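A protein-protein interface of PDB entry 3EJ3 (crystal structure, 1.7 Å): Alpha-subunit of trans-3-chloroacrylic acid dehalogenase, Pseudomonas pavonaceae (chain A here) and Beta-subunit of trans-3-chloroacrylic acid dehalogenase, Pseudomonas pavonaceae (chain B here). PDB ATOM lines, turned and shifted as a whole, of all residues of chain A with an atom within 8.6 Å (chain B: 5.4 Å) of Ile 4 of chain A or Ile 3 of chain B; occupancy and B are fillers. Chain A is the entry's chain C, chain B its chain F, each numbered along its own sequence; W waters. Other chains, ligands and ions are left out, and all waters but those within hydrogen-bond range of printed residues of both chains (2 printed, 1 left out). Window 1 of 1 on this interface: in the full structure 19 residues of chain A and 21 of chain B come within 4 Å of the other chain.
N of His 6 of chain B sits at hydrogen-bond distance from O of Met 3 of chain A, 2.8 Å away.
N of Ser 5 of chain A lies within hydrogen-bond range of O of Glu 4 of chain B, at 2.9 Å.
The backbone NH (N) of Asp 7 of chain A lies within hydrogen-bond range of the backbone carbonyl oxygen (O) of Phe 2 of chain B (2.9 Å).
The side-chain hydroxyl of Thr 27 of chain B lies within hydrogen-bond range of the backbone carbonyl oxygen of Val 23 of chain B, 2.8 Å away.
O of Pro 1 of chain B lies within hydrogen-bond range of N of Asn 39 of chain B (3.0 Å).
The backbone NH (N) of Cys 5 of chain B is in hydrogen-bond range of the backbone carbonyl oxygen (O) of Leu 41 of chain B (2.9 Å).
The backbone carbonyl oxygen (O) of Ile 28 of chain A is in hydrogen-bond range of the side-chain hydroxyl (OG1) of Thr 32 of chain A.
The backbone carbonyl oxygen of Cys 6 of chain A sits at hydrogen-bond distance from the backbone NH of Arg 44 of chain A.
OG of Ser 5 of chain A is in hydrogen-bond range of NH1 of Arg 44 of chain A, at 3.4 Å.
O of Met 3 of chain A touches O of Glu 4 of chain B, at 3.9 Å.
Met 3 of chain A touches Cys 5 of chain B (O to C, 3.7 Å).
CG2 of Ile 4 of chain A touches CG2 of Ile 3 of chain B, at 3.8 Å.
Ile 4 of chain A touches Glu 4 of chain B (CA to O, 3.3 Å).
O of Phe 2 of chain B touches O of Ser 5 of chain A, 3.6 Å away.
Ser 5 of chain A touches Ile 3 of chain B.
Cys 6 of chain A touches Phe 2 of chain B (CA to O, 3.3 Å).
Pro 1 of chain B touches Asp 7 of chain A (CA to O, 3.3 Å).
CD1 of Leu 20 of chain A touches OG1 of Thr 27 of chain B, at 3.97 Å.
Cys 5 of chain B touches Ile 28 of chain A (SG to CD1, 3.9 Å).
Of the printed residues of chain B, Ile 4 of chain A touches Ile 3, Glu 4 and Cys 5.
Of the printed residues of chain B, Cys 6 of chain A touches Phe 2 (3.3 Å).
Printed residues of chain A within 4 Å of Ile 3 of chain B: Ile 4 (3.8 Å) and Ser 5 (3.2 Å).
Printed residues of chain A within 4 Å of Thr 27 of chain B: Leu 20 (3.97 Å).
Asn 39 of chain B touches none of the printed residues of chain A.
The nearest printed residue of chain B that does not touch Ile 4 of chain A is His 6 of chain B (4.1 Å).
The nearest printed residue of chain A that does not touch Ile 3 of chain B is Cys 6 of chain A (4.4 Å).
The nearest printed residue of chain A that does not touch His 6 of chain B is Ile 4 of chain A (4.1 Å).
Of the 13 printed residues of chain B, 9 touch a printed residue of chain A.
Printed residues of chain B that touch a printed residue of chain A: Pro 1, Phe 2, Ile 3, Glu 4, Cys 5, His 6, Ile 7, Val 23 and Thr 27.
Hydrophobic or aromatic side chains of chain B that line the printed part of chain A: Pro 1, Ile 3, His 6, Ile 7 and Val 23.
Along chain A the printed residues that touch a printed residue of chain B span positions 2 to 32.
Among the printed residues, 17 pairs touch across the chains.
Among the printed residues, no Asp or Glu carboxylate lies within 4 Å of a Lys or Arg side-chain nitrogen of the other chain.
Water W1 lies within hydrogen-bond range of the side-chain carboxylate (OD2) of Asp 7 of chain A (2.7 Å), the side-chain hydroxyl (OG) of Ser 5 of chain A (2.7 Å) and the backbone carbonyl oxygen (O) of Phe 2 of chain B (2.9 Å).
Water W2 lies within hydrogen-bond range of OG of Ser 5 of chain A and NE2 of His 6 of chain B.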
ATOM      1  N   PRO A   2      17.844  14.034 -14.705  1.00  0.00           N
ATOM      2  CA  PRO A   2      17.310  15.325 -15.165  1.00  0.00           C
ATOM      3  C   PRO A   2      16.807  15.247 -16.613  1.00  0.00           C
ATOM      4  O   PRO A   2      17.181  14.348 -17.339  1.00  0.00           O
ATOM      5  CB  PRO A   2      18.512  16.249 -15.083  1.00  0.00           C
ATOM      6  CG  PRO A   2      19.344  15.669 -13.955  1.00  0.00           C
ATOM      7  CD  PRO A   2      19.196  14.177 -14.130  1.00  0.00           C
ATOM      8  N   MET A   3      15.932  16.171 -17.005  1.00  0.00           N
ATOM      9  CA  MET A   3      15.413  16.175 -18.370  1.00  0.00           C
ATOM     10  C   MET A   3      15.604  17.549 -18.929  1.00  0.00           C
ATOM     11  O   MET A   3      15.257  18.538 -18.245  1.00  0.00           O
ATOM     12  CB  MET A   3      13.923  15.858 -18.385  1.00  0.00           C
ATOM     13  CG  MET A   3      13.570  14.505 -17.803  1.00  0.00           C
ATOM     14  SD  MET A   3      13.430  14.566 -16.005  1.00  0.00           S
ATOM     15  CE  MET A   3      12.537  13.013 -15.699  1.00  0.00           C
ATOM     16  N   ILE A   4      16.062  17.635 -20.175  1.00  0.00           N
ATOM     17  CA  ILE A   4      16.287  18.978 -20.752  1.00  0.00           C
ATOM     18  C   ILE A   4      15.556  19.051 -22.077  1.00  0.00           C
ATOM     19  O   ILE A   4      15.559  18.093 -22.813  1.00  0.00           O
ATOM     20  CB  ILE A   4      17.801  19.198 -21.011  1.00  0.00           C
ATOM     21  CG1 ILE A   4      18.628  18.820 -19.781  1.00  0.00           C
ATOM     22  CG2 ILE A   4      18.122  20.607 -21.592  1.00  0.00           C
ATOM     23  CD1 ILE A   4      18.299  19.575 -18.455  1.00  0.00           C
ATOM     24  N   SER A   5      14.955  20.198 -22.396  1.00  0.00           N
ATOM     25  CA  SER A   5      14.381  20.348 -23.706  1.00  0.00           C
ATOM     26  C   SER A   5      14.874  21.632 -24.338  1.00  0.00           C
ATOM     27  O   SER A   5      15.206  22.593 -23.638  1.00  0.00           O
ATOM     28  CB  SER A   5      12.848  20.305 -23.648  1.00  0.00           C
ATOM     29  OG  SER A   5      12.334  21.408 -22.899  1.00  0.00           O
ATOM     30  N   CYS A   6      14.920  21.649 -25.657  1.00  0.00           N
ATOM     31  CA  CYS A   6      15.314  22.864 -26.374  1.00  0.00           C
ATOM     32  C   CYS A   6      14.337  23.078 -27.502  1.00  0.00           C
ATOM     33  O   CYS A   6      14.308  22.275 -28.422  1.00  0.00           O
ATOM     34  CB  CYS A   6      16.720  22.697 -26.928  1.00  0.00           C
ATOM     35  SG  CYS A   6      17.277  24.031 -28.018  1.00  0.00           S
ATOM     36  N   ASP A   7      13.576  24.176 -27.455  1.00  0.00           N
ATOM     37  CA  ASP A   7      12.708  24.559 -28.577  1.00  0.00           C
ATOM     38  C   ASP A   7      13.495  25.501 -29.473  1.00  0.00           C
ATOM     39  O   ASP A   7      13.980  26.540 -29.031  1.00  0.00           O
ATOM     40  CB  ASP A   7      11.429  25.264 -28.093  1.00  0.00           C
ATOM     41  CG  ASP A   7      10.407  24.295 -27.482  1.00  0.00           C
ATOM     42  OD1 ASP A   7       9.490  23.890 -28.203  1.00  0.00           O
ATOM     43  OD2 ASP A   7      10.494  23.955 -26.280  1.00  0.00           O
ATOM     44  N   MET A   8      13.632  25.143 -30.739  1.00  0.00           N
ATOM     45  CA  MET A   8      14.303  26.045 -31.687  1.00  0.00           C
ATOM     46  C   MET A   8      13.818  25.781 -33.096  1.00  0.00           C
ATOM     47  O   MET A   8      13.162  24.778 -33.365  1.00  0.00           O
ATOM     48  CB  MET A   8      15.813  25.882 -31.647  1.00  0.00           C
ATOM     49  CG  MET A   8      16.304  24.521 -32.080  1.00  0.00           C
ATOM     50  SD  MET A   8      18.111  24.644 -31.952  1.00  0.00           S
ATOM     51  CE  MET A   8      18.573  22.993 -32.401  1.00  0.00           C
ATOM     52  N   LEU A  20      25.420  20.706 -29.355  1.00  0.00           N
ATOM     53  CA  LEU A  20      24.515  21.274 -28.354  1.00  0.00           C
ATOM     54  C   LEU A  20      24.301  20.266 -27.231  1.00  0.00           C
ATOM     55  O   LEU A  20      24.380  20.623 -26.058  1.00  0.00           O
ATOM     56  CB  LEU A  20      23.153  21.585 -29.012  1.00  0.00           C
ATOM     57  CG  LEU A  20      22.093  22.264 -28.120  1.00  0.00           C
ATOM     58  CD1 LEU A  20      22.607  23.548 -27.468  1.00  0.00           C
ATOM     59  CD2 LEU A  20      20.869  22.531 -28.987  1.00  0.00           C
ATOM     60  N   SER A  21      24.030  19.013 -27.591  1.00  0.00           N
ATOM     61  CA  SER A  21      23.778  17.972 -26.572  1.00  0.00           C
ATOM     62  C   SER A  21      25.004  17.717 -25.683  1.00  0.00           C
ATOM     63  O   SER A  21      24.886  17.611 -24.455  1.00  0.00           O
ATOM     64  CB  SER A  21      23.294  16.689 -27.213  1.00  0.00           C
ATOM     65  OG  SER A  21      24.392  15.968 -27.734  1.00  0.00           O
ATOM     66  N   GLY A  23      27.404  19.821 -24.919  1.00  0.00           N
ATOM     67  CA  GLY A  23      27.565  20.960 -24.019  1.00  0.00           C
ATOM     68  C   GLY A  23      26.542  20.951 -22.902  1.00  0.00           C
ATOM     69  O   GLY A  23      26.885  21.137 -21.730  1.00  0.00           O
ATOM     70  N   LEU A  24      25.273  20.767 -23.269  1.00  0.00           N
ATOM     71  CA  LEU A  24      24.209  20.776 -22.267  1.00  0.00           C
ATOM     72  C   LEU A  24      24.329  19.611 -21.275  1.00  0.00           C
ATOM     73  O   LEU A  24      24.159  19.797 -20.082  1.00  0.00           O
ATOM     74  CB  LEU A  24      22.825  20.804 -22.942  1.00  0.00           C
ATOM     75  CG  LEU A  24      22.495  22.131 -23.648  1.00  0.00           C
ATOM     76  CD1 LEU A  24      21.175  21.927 -24.371  1.00  0.00           C
ATOM     77  CD2 LEU A  24      22.478  23.402 -22.743  1.00  0.00           C
ATOM     78  N   LEU A  25      24.597  18.404 -21.763  1.00  0.00           N
ATOM     79  CA  LEU A  25      24.801  17.271 -20.848  1.00  0.00           C
ATOM     80  C   LEU A  25      25.933  17.558 -19.860  1.00  0.00           C
ATOM     81  O   LEU A  25      25.808  17.302 -18.644  1.00  0.00           O
ATOM     82  CB  LEU A  25      25.023  15.964 -21.614  1.00  0.00           C
ATOM     83  CG  LEU A  25      23.805  15.073 -21.937  1.00  0.00           C
ATOM     84  CD1 LEU A  25      22.600  15.821 -22.505  1.00  0.00           C
ATOM     85  CD2 LEU A  25      24.230  13.918 -22.878  1.00  0.00           C
ATOM     86  N   ARG A  26      27.026  18.114 -20.374  1.00  0.00           N
ATOM     87  CA  ARG A  26      28.162  18.453 -19.534  1.00  0.00           C
ATOM     88  C   ARG A  26      27.782  19.447 -18.446  1.00  0.00           C
ATOM     89  O   ARG A  26      28.074  19.219 -17.282  1.00  0.00           O
ATOM     90  CB  ARG A  26      29.335  18.987 -20.358  1.00  0.00           C
ATOM     91  CG  ARG A  26      30.505  19.517 -19.496  1.00  0.00           C
ATOM     92  CD  ARG A  26      31.699  19.954 -20.367  1.00  0.00           C
ATOM     93  NE  ARG A  26      31.437  21.217 -21.074  1.00  0.00           N
ATOM     94  CZ  ARG A  26      31.149  21.324 -22.376  1.00  0.00           C
ATOM     95  NH1 ARG A  26      31.082  20.244 -23.156  1.00  0.00           N
ATOM     96  NH2 ARG A  26      30.926  22.522 -22.909  1.00  0.00           N
ATOM     97  N   VAL A  27      27.121  20.543 -18.814  1.00  0.00           N
ATOM     98  CA  VAL A  27      26.783  21.560 -17.821  1.00  0.00           C
ATOM     99  C   VAL A  27      25.762  21.085 -16.794  1.00  0.00           C
ATOM    100  O   VAL A  27      25.882  21.397 -15.617  1.00  0.00           O
ATOM    101  CB  VAL A  27      26.390  22.971 -18.418  1.00  0.00           C
ATOM    102  CG1 VAL A  27      27.512  23.486 -19.377  1.00  0.00           C
ATOM    103  CG2 VAL A  27      25.098  22.923 -19.137  1.00  0.00           C
ATOM    104  N   ILE A  28      24.776  20.318 -17.236  1.00  0.00           N
ATOM    105  CA  ILE A  28      23.761  19.817 -16.317  1.00  0.00           C
ATOM    106  C   ILE A  28      24.369  18.764 -15.395  1.00  0.00           C
ATOM    107  O   ILE A  28      24.062  18.716 -14.190  1.00  0.00           O
ATOM    108  CB  ILE A  28      22.547  19.263 -17.092  1.00  0.00           C
ATOM    109  CG1 ILE A  28      21.801  20.433 -17.738  1.00  0.00           C
ATOM    110  CG2 ILE A  28      21.605  18.490 -16.180  1.00  0.00           C
ATOM    111  CD1 ILE A  28      21.173  21.347 -16.715  1.00  0.00           C
ATOM    112  N   SER A  29      25.222  17.909 -15.954  1.00  0.00           N
ATOM    113  CA  SER A  29      25.889  16.900 -15.122  1.00  0.00           C
ATOM    114  C   SER A  29      26.684  17.561 -13.998  1.00  0.00           C
ATOM    115  O   SER A  29      26.562  17.191 -12.823  1.00  0.00           O
ATOM    116  CB  SER A  29      26.801  16.004 -15.954  1.00  0.00           C
ATOM    117  OG  SER A  29      27.570  15.157 -15.090  1.00  0.00           O
ATOM    118  N   THR A  32      24.222  19.104 -11.352  1.00  0.00           N
ATOM    119  CA  THR A  32      23.287  18.243 -10.642  1.00  0.00           C
ATOM    120  C   THR A  32      23.991  17.116  -9.921  1.00  0.00           C
ATOM    121  O   THR A  32      23.389  16.448  -9.081  1.00  0.00           O
ATOM    122  CB  THR A  32      22.243  17.642 -11.576  1.00  0.00           C
ATOM    123  OG1 THR A  32      22.875  16.824 -12.572  1.00  0.00           O
ATOM    124  CG2 THR A  32      21.421  18.750 -12.232  1.00  0.00           C
ATOM    125  N   ASN A  38      22.228   9.819 -17.144  1.00  0.00           N
ATOM    126  CA  ASN A  38      20.986  10.098 -16.421  1.00  0.00           C
ATOM    127  C   ASN A  38      20.276  11.361 -16.865  1.00  0.00           C
ATOM    128  O   ASN A  38      19.303  11.775 -16.231  1.00  0.00           O
ATOM    129  CB  ASN A  38      21.259  10.207 -14.933  1.00  0.00           C
ATOM    130  CG  ASN A  38      21.509   8.868 -14.315  1.00  0.00           C
ATOM    131  OD1 ASN A  38      21.433   7.841 -15.001  1.00  0.00           O
ATOM    132  ND2 ASN A  38      21.784   8.856 -13.018  1.00  0.00           N
ATOM    133  N   ILE A  39      20.770  11.974 -17.936  1.00  0.00           N
ATOM    134  CA  ILE A  39      20.197  13.233 -18.403  1.00  0.00           C
ATOM    135  C   ILE A  39      19.534  13.048 -19.766  1.00  0.00           C
ATOM    136  O   ILE A  39      20.243  12.848 -20.760  1.00  0.00           O
ATOM    137  CB  ILE A  39      21.289  14.327 -18.494  1.00  0.00           C
ATOM    138  CG1 ILE A  39      21.917  14.580 -17.111  1.00  0.00           C
ATOM    139  CG2 ILE A  39      20.722  15.623 -19.136  1.00  0.00           C
ATOM    140  CD1 ILE A  39      23.282  15.262 -17.182  1.00  0.00           C
ATOM    141  N   PHE A  40      18.195  13.122 -19.828  1.00  0.00           N
ATOM    142  CA  PHE A  40      17.452  12.977 -21.089  1.00  0.00           C
ATOM    143  C   PHE A  40      17.418  14.354 -21.779  1.00  0.00           C
ATOM    144  O   PHE A  40      17.226  15.356 -21.088  1.00  0.00           O
ATOM    145  CB  PHE A  40      16.015  12.500 -20.800  1.00  0.00           C
ATOM    146  CG  PHE A  40      15.101  12.596 -21.990  1.00  0.00           C
ATOM    147  CD1 PHE A  40      15.065  11.567 -22.940  1.00  0.00           C
ATOM    148  CD2 PHE A  40      14.305  13.723 -22.200  1.00  0.00           C
ATOM    149  CE1 PHE A  40      14.242  11.645 -24.051  1.00  0.00           C
ATOM    150  CE2 PHE A  40      13.488  13.802 -23.348  1.00  0.00           C
ATOM    151  CZ  PHE A  40      13.463  12.775 -24.253  1.00  0.00           C
ATOM    152  N   PHE A  41      17.559  14.408 -23.107  1.00  0.00           N
ATOM    153  CA  PHE A  41      17.519  15.675 -23.852  1.00  0.00           C
ATOM    154  C   PHE A  41      16.689  15.509 -25.097  1.00  0.00           C
ATOM    155  O   PHE A  41      16.810  14.484 -25.797  1.00  0.00           O
ATOM    156  CB  PHE A  41      18.945  16.109 -24.223  1.00  0.00           C
ATOM    157  CG  PHE A  41      19.031  17.388 -25.035  1.00  0.00           C
ATOM    158  CD1 PHE A  41      18.316  18.541 -24.665  1.00  0.00           C
ATOM    159  CD2 PHE A  41      19.859  17.451 -26.152  1.00  0.00           C
ATOM    160  CE1 PHE A  41      18.414  19.738 -25.419  1.00  0.00           C
ATOM    161  CE2 PHE A  41      19.970  18.642 -26.916  1.00  0.00           C
ATOM    162  CZ  PHE A  41      19.252  19.792 -26.533  1.00  0.00           C
ATOM    163  N   VAL A  42      15.776  16.468 -25.319  1.00  0.00           N
ATOM    164  CA  VAL A  42      14.994  16.497 -26.564  1.00  0.00           C
ATOM    165  C   VAL A  42      15.005  17.883 -27.200  1.00  0.00           C
ATOM    166  O   VAL A  42      14.791  18.896 -26.513  1.00  0.00           O
ATOM    167  CB  VAL A  42      13.528  16.031 -26.363  1.00  0.00           C
ATOM    168  CG1 VAL A  42      12.823  16.857 -25.277  1.00  0.00           C
ATOM    169  CG2 VAL A  42      12.759  16.058 -27.720  1.00  0.00           C
ATOM    170  N   ILE A  43      15.274  17.919 -28.501  1.00  0.00           N
ATOM    171  CA  ILE A  43      15.165  19.142 -29.267  1.00  0.00           C
ATOM    172  C   ILE A  43      13.803  19.125 -29.931  1.00  0.00           C
ATOM    173  O   ILE A  43      13.441  18.150 -30.559  1.00  0.00           O
ATOM    174  CB  ILE A  43      16.269  19.215 -30.349  1.00  0.00           C
ATOM    175  CG1 ILE A  43      17.625  19.370 -29.654  1.00  0.00           C
ATOM    176  CG2 ILE A  43      15.993  20.350 -31.315  1.00  0.00           C
ATOM    177  CD1 ILE A  43      18.827  18.947 -30.485  1.00  0.00           C
ATOM    178  N   ARG A  44      13.052  20.223 -29.795  1.00  0.00           N
ATOM    179  CA  ARG A  44      11.738  20.323 -30.408  1.00  0.00           C
ATOM    180  C   ARG A  44      11.836  21.409 -31.474  1.00  0.00           C
ATOM    181  O   ARG A  44      12.109  22.555 -31.157  1.00  0.00           O
ATOM    182  CB  ARG A  44      10.680  20.722 -29.370  1.00  0.00           C
ATOM    183  CG  ARG A  44      10.579  19.738 -28.210  1.00  0.00           C
ATOM    184  CD  ARG A  44       9.490  20.178 -27.327  1.00  0.00           C
ATOM    185  NE  ARG A  44       9.315  19.367 -26.113  1.00  0.00           N
ATOM    186  CZ  ARG A  44       9.325  19.840 -24.877  1.00  0.00           C
ATOM    187  NH1 ARG A  44       9.489  21.152 -24.651  1.00  0.00           N
ATOM    188  NH2 ARG A  44       9.095  19.016 -23.859  1.00  0.00           N
ATOM    189  N   PRO B   1      16.657  30.161 -29.135  1.00  0.00           N
ATOM    190  CA  PRO B   1      16.226  28.898 -28.548  1.00  0.00           C
ATOM    191  C   PRO B   1      15.746  29.058 -27.114  1.00  0.00           C
ATOM    192  O   PRO B   1      16.168  30.003 -26.420  1.00  0.00           O
ATOM    193  CB  PRO B   1      17.504  28.037 -28.561  1.00  0.00           C
ATOM    194  CG  PRO B   1      18.535  28.814 -29.307  1.00  0.00           C
ATOM    195  CD  PRO B   1      18.122  30.259 -29.211  1.00  0.00           C
ATOM    196  N   PHE B   2      14.881  28.140 -26.681  1.00  0.00           N
ATOM    197  CA  PHE B   2      14.338  28.136 -25.326  1.00  0.00           C
ATOM    198  C   PHE B   2      14.707  26.803 -24.699  1.00  0.00           C
ATOM    199  O   PHE B   2      14.234  25.741 -25.149  1.00  0.00           O
ATOM    200  CB  PHE B   2      12.819  28.248 -25.386  1.00  0.00           C
ATOM    201  CG  PHE B   2      12.127  28.017 -24.072  1.00  0.00           C
ATOM    202  CD1 PHE B   2      12.636  28.552 -22.891  1.00  0.00           C
ATOM    203  CD2 PHE B   2      10.962  27.257 -24.020  1.00  0.00           C
ATOM    204  CE1 PHE B   2      11.974  28.343 -21.661  1.00  0.00           C
ATOM    205  CE2 PHE B   2      10.286  27.072 -22.795  1.00  0.00           C
ATOM    206  CZ  PHE B   2      10.808  27.595 -21.629  1.00  0.00           C
ATOM    207  N   ILE B   3      15.527  26.863 -23.650  1.00  0.00           N
ATOM    208  CA  ILE B   3      16.042  25.643 -23.005  1.00  0.00           C
ATOM    209  C   ILE B   3      15.404  25.487 -21.631  1.00  0.00           C
ATOM    210  O   ILE B   3      15.543  26.373 -20.790  1.00  0.00           O
ATOM    211  CB  ILE B   3      17.580  25.655 -22.860  1.00  0.00           C
ATOM    212  CG1 ILE B   3      18.285  25.921 -24.205  1.00  0.00           C
ATOM    213  CG2 ILE B   3      18.076  24.310 -22.349  1.00  0.00           C
ATOM    214  CD1 ILE B   3      18.529  27.378 -24.513  1.00  0.00           C
ATOM    215  N   GLU B   4      14.698  24.381 -21.424  1.00  0.00           N
ATOM    216  CA  GLU B   4      14.022  24.104 -20.140  1.00  0.00           C
ATOM    217  C   GLU B   4      14.788  22.978 -19.474  1.00  0.00           C
ATOM    218  O   GLU B   4      15.016  21.928 -20.086  1.00  0.00           O
ATOM    219  CB  GLU B   4      12.542  23.740 -20.362  1.00  0.00           C
ATOM    220  CG  GLU B   4      11.705  23.573 -19.108  1.00  0.00           C
ATOM    221  CD  GLU B   4      10.176  23.552 -19.378  1.00  0.00           C
ATOM    222  OE1 GLU B   4       9.731  24.011 -20.458  1.00  0.00           O
ATOM    223  OE2 GLU B   4       9.431  23.112 -18.459  1.00  0.00           O
ATOM    224  N   CYS B   5      15.188  23.189 -18.223  1.00  0.00           N
ATOM    225  CA  CYS B   5      15.975  22.192 -17.515  1.00  0.00           C
ATOM    226  C   CYS B   5      15.206  21.728 -16.298  1.00  0.00           C
ATOM    227  O   CYS B   5      14.941  22.520 -15.404  1.00  0.00           O
ATOM    228  CB  CYS B   5      17.308  22.760 -17.038  1.00  0.00           C
ATOM    229  SG  CYS B   5      18.324  23.427 -18.356  1.00  0.00           S
ATOM    230  N   HIS B   6      14.897  20.447 -16.252  1.00  0.00           N
ATOM    231  CA  HIS B   6      14.133  19.855 -15.129  1.00  0.00           C
ATOM    232  C   HIS B   6      15.139  19.142 -14.250  1.00  0.00           C
ATOM    233  O   HIS B   6      15.763  18.164 -14.682  1.00  0.00           O
ATOM    234  CB  HIS B   6      13.110  18.840 -15.654  1.00  0.00           C
ATOM    235  CG  HIS B   6      12.059  19.446 -16.520  1.00  0.00           C
ATOM    236  ND1 HIS B   6      10.999  20.153 -16.001  1.00  0.00           N
ATOM    237  CD2 HIS B   6      11.927  19.494 -17.866  1.00  0.00           C
ATOM    238  CE1 HIS B   6      10.253  20.612 -16.988  1.00  0.00           C
ATOM    239  NE2 HIS B   6      10.776  20.203 -18.127  1.00  0.00           N
ATOM    240  N   ILE B   7      15.321  19.645 -13.034  1.00  0.00           N
ATOM    241  CA  ILE B   7      16.330  19.097 -12.141  1.00  0.00           C
ATOM    242  C   ILE B   7      15.763  18.908 -10.749  1.00  0.00           C
ATOM    243  O   ILE B   7      14.721  19.461 -10.409  1.00  0.00           O
ATOM    244  CB  ILE B   7      17.534  20.048 -12.054  1.00  0.00           C
ATOM    245  CG1 ILE B   7      17.112  21.412 -11.480  1.00  0.00           C
ATOM    246  CG2 ILE B   7      18.217  20.207 -13.473  1.00  0.00           C
ATOM    247  CD1 ILE B   7      18.384  22.356 -11.098  1.00  0.00           C
ATOM    248  N   VAL B  23      24.425  27.282 -19.491  1.00  0.00           N
ATOM    249  CA  VAL B  23      23.496  26.913 -20.592  1.00  0.00           C
ATOM    250  C   VAL B  23      23.542  27.955 -21.756  1.00  0.00           C
ATOM    251  O   VAL B  23      23.616  27.590 -22.927  1.00  0.00           O
ATOM    252  CB  VAL B  23      22.033  26.698 -20.060  1.00  0.00           C
ATOM    253  CG1 VAL B  23      21.018  26.559 -21.224  1.00  0.00           C
ATOM    254  CG2 VAL B  23      21.958  25.471 -19.172  1.00  0.00           C
ATOM    255  N   THR B  27      24.989  26.983 -25.504  1.00  0.00           N
ATOM    256  CA  THR B  27      24.116  27.199 -26.655  1.00  0.00           C
ATOM    257  C   THR B  27      24.771  28.108 -27.688  1.00  0.00           C
ATOM    258  O   THR B  27      24.813  27.775 -28.878  1.00  0.00           O
ATOM    259  CB  THR B  27      22.742  27.733 -26.167  1.00  0.00           C
ATOM    260  OG1 THR B  27      22.262  26.793 -25.213  1.00  0.00           O
ATOM    261  CG2 THR B  27      21.746  27.838 -27.327  1.00  0.00           C
ATOM    262  N   ILE B  38      18.571  33.928 -26.294  1.00  0.00           N
ATOM    263  CA  ILE B  38      18.521  32.604 -25.673  1.00  0.00           C
ATOM    264  C   ILE B  38      17.740  32.742 -24.374  1.00  0.00           C
ATOM    265  O   ILE B  38      18.022  33.619 -23.558  1.00  0.00           O
ATOM    266  CB  ILE B  38      19.955  32.082 -25.342  1.00  0.00           C
ATOM    267  CG1 ILE B  38      20.739  31.855 -26.647  1.00  0.00           C
ATOM    268  CG2 ILE B  38      19.885  30.812 -24.491  1.00  0.00           C
ATOM    269  CD1 ILE B  38      22.265  31.565 -26.438  1.00  0.00           C
ATOM    270  N   ASN B  39      16.757  31.872 -24.196  1.00  0.00           N
ATOM    271  CA  ASN B  39      15.893  31.905 -23.021  1.00  0.00           C
ATOM    272  C   ASN B  39      16.045  30.599 -22.280  1.00  0.00           C
ATOM    273  O   ASN B  39      16.079  29.528 -22.883  1.00  0.00           O
ATOM    274  CB  ASN B  39      14.463  32.080 -23.492  1.00  0.00           C
ATOM    275  CG  ASN B  39      14.304  33.277 -24.418  1.00  0.00           C
ATOM    276  OD1 ASN B  39      14.336  34.427 -23.967  1.00  0.00           O
ATOM    277  ND2 ASN B  39      14.149  33.020 -25.719  1.00  0.00           N
ATOM    278  N   VAL B  40      16.164  30.678 -20.964  1.00  0.00           N
ATOM    279  CA  VAL B  40      16.386  29.503 -20.152  1.00  0.00           C
ATOM    280  C   VAL B  40      15.414  29.499 -18.959  1.00  0.00           C
ATOM    281  O   VAL B  40      15.174  30.537 -18.323  1.00  0.00           O
ATOM    282  CB  VAL B  40      17.818  29.471 -19.613  1.00  0.00           C
ATOM    283  CG1 VAL B  40      18.038  28.197 -18.831  1.00  0.00           C
ATOM    284  CG2 VAL B  40      18.791  29.583 -20.767  1.00  0.00           C
ATOM    285  N   LEU B  41      14.868  28.329 -18.672  1.00  0.00           N
ATOM    286  CA  LEU B  41      13.974  28.136 -17.529  1.00  0.00           C
ATOM    287  C   LEU B  41      14.464  26.948 -16.758  1.00  0.00           C
ATOM    288  O   LEU B  41      14.550  25.843 -17.301  1.00  0.00           O
ATOM    289  CB  LEU B  41      12.539  27.884 -18.013  1.00  0.00           C
ATOM    290  CG  LEU B  41      11.492  27.554 -16.913  1.00  0.00           C
ATOM    291  CD1 LEU B  41      11.285  28.715 -15.907  1.00  0.00           C
ATOM    292  CD2 LEU B  41      10.133  27.141 -17.551  1.00  0.00           C
HETATM  293  O   HOH W   1      12.287  23.715 -24.321  1.00  0.00           O
HETATM  294  O   HOH W   2      10.477  20.498 -21.004  1.00  0.00           O
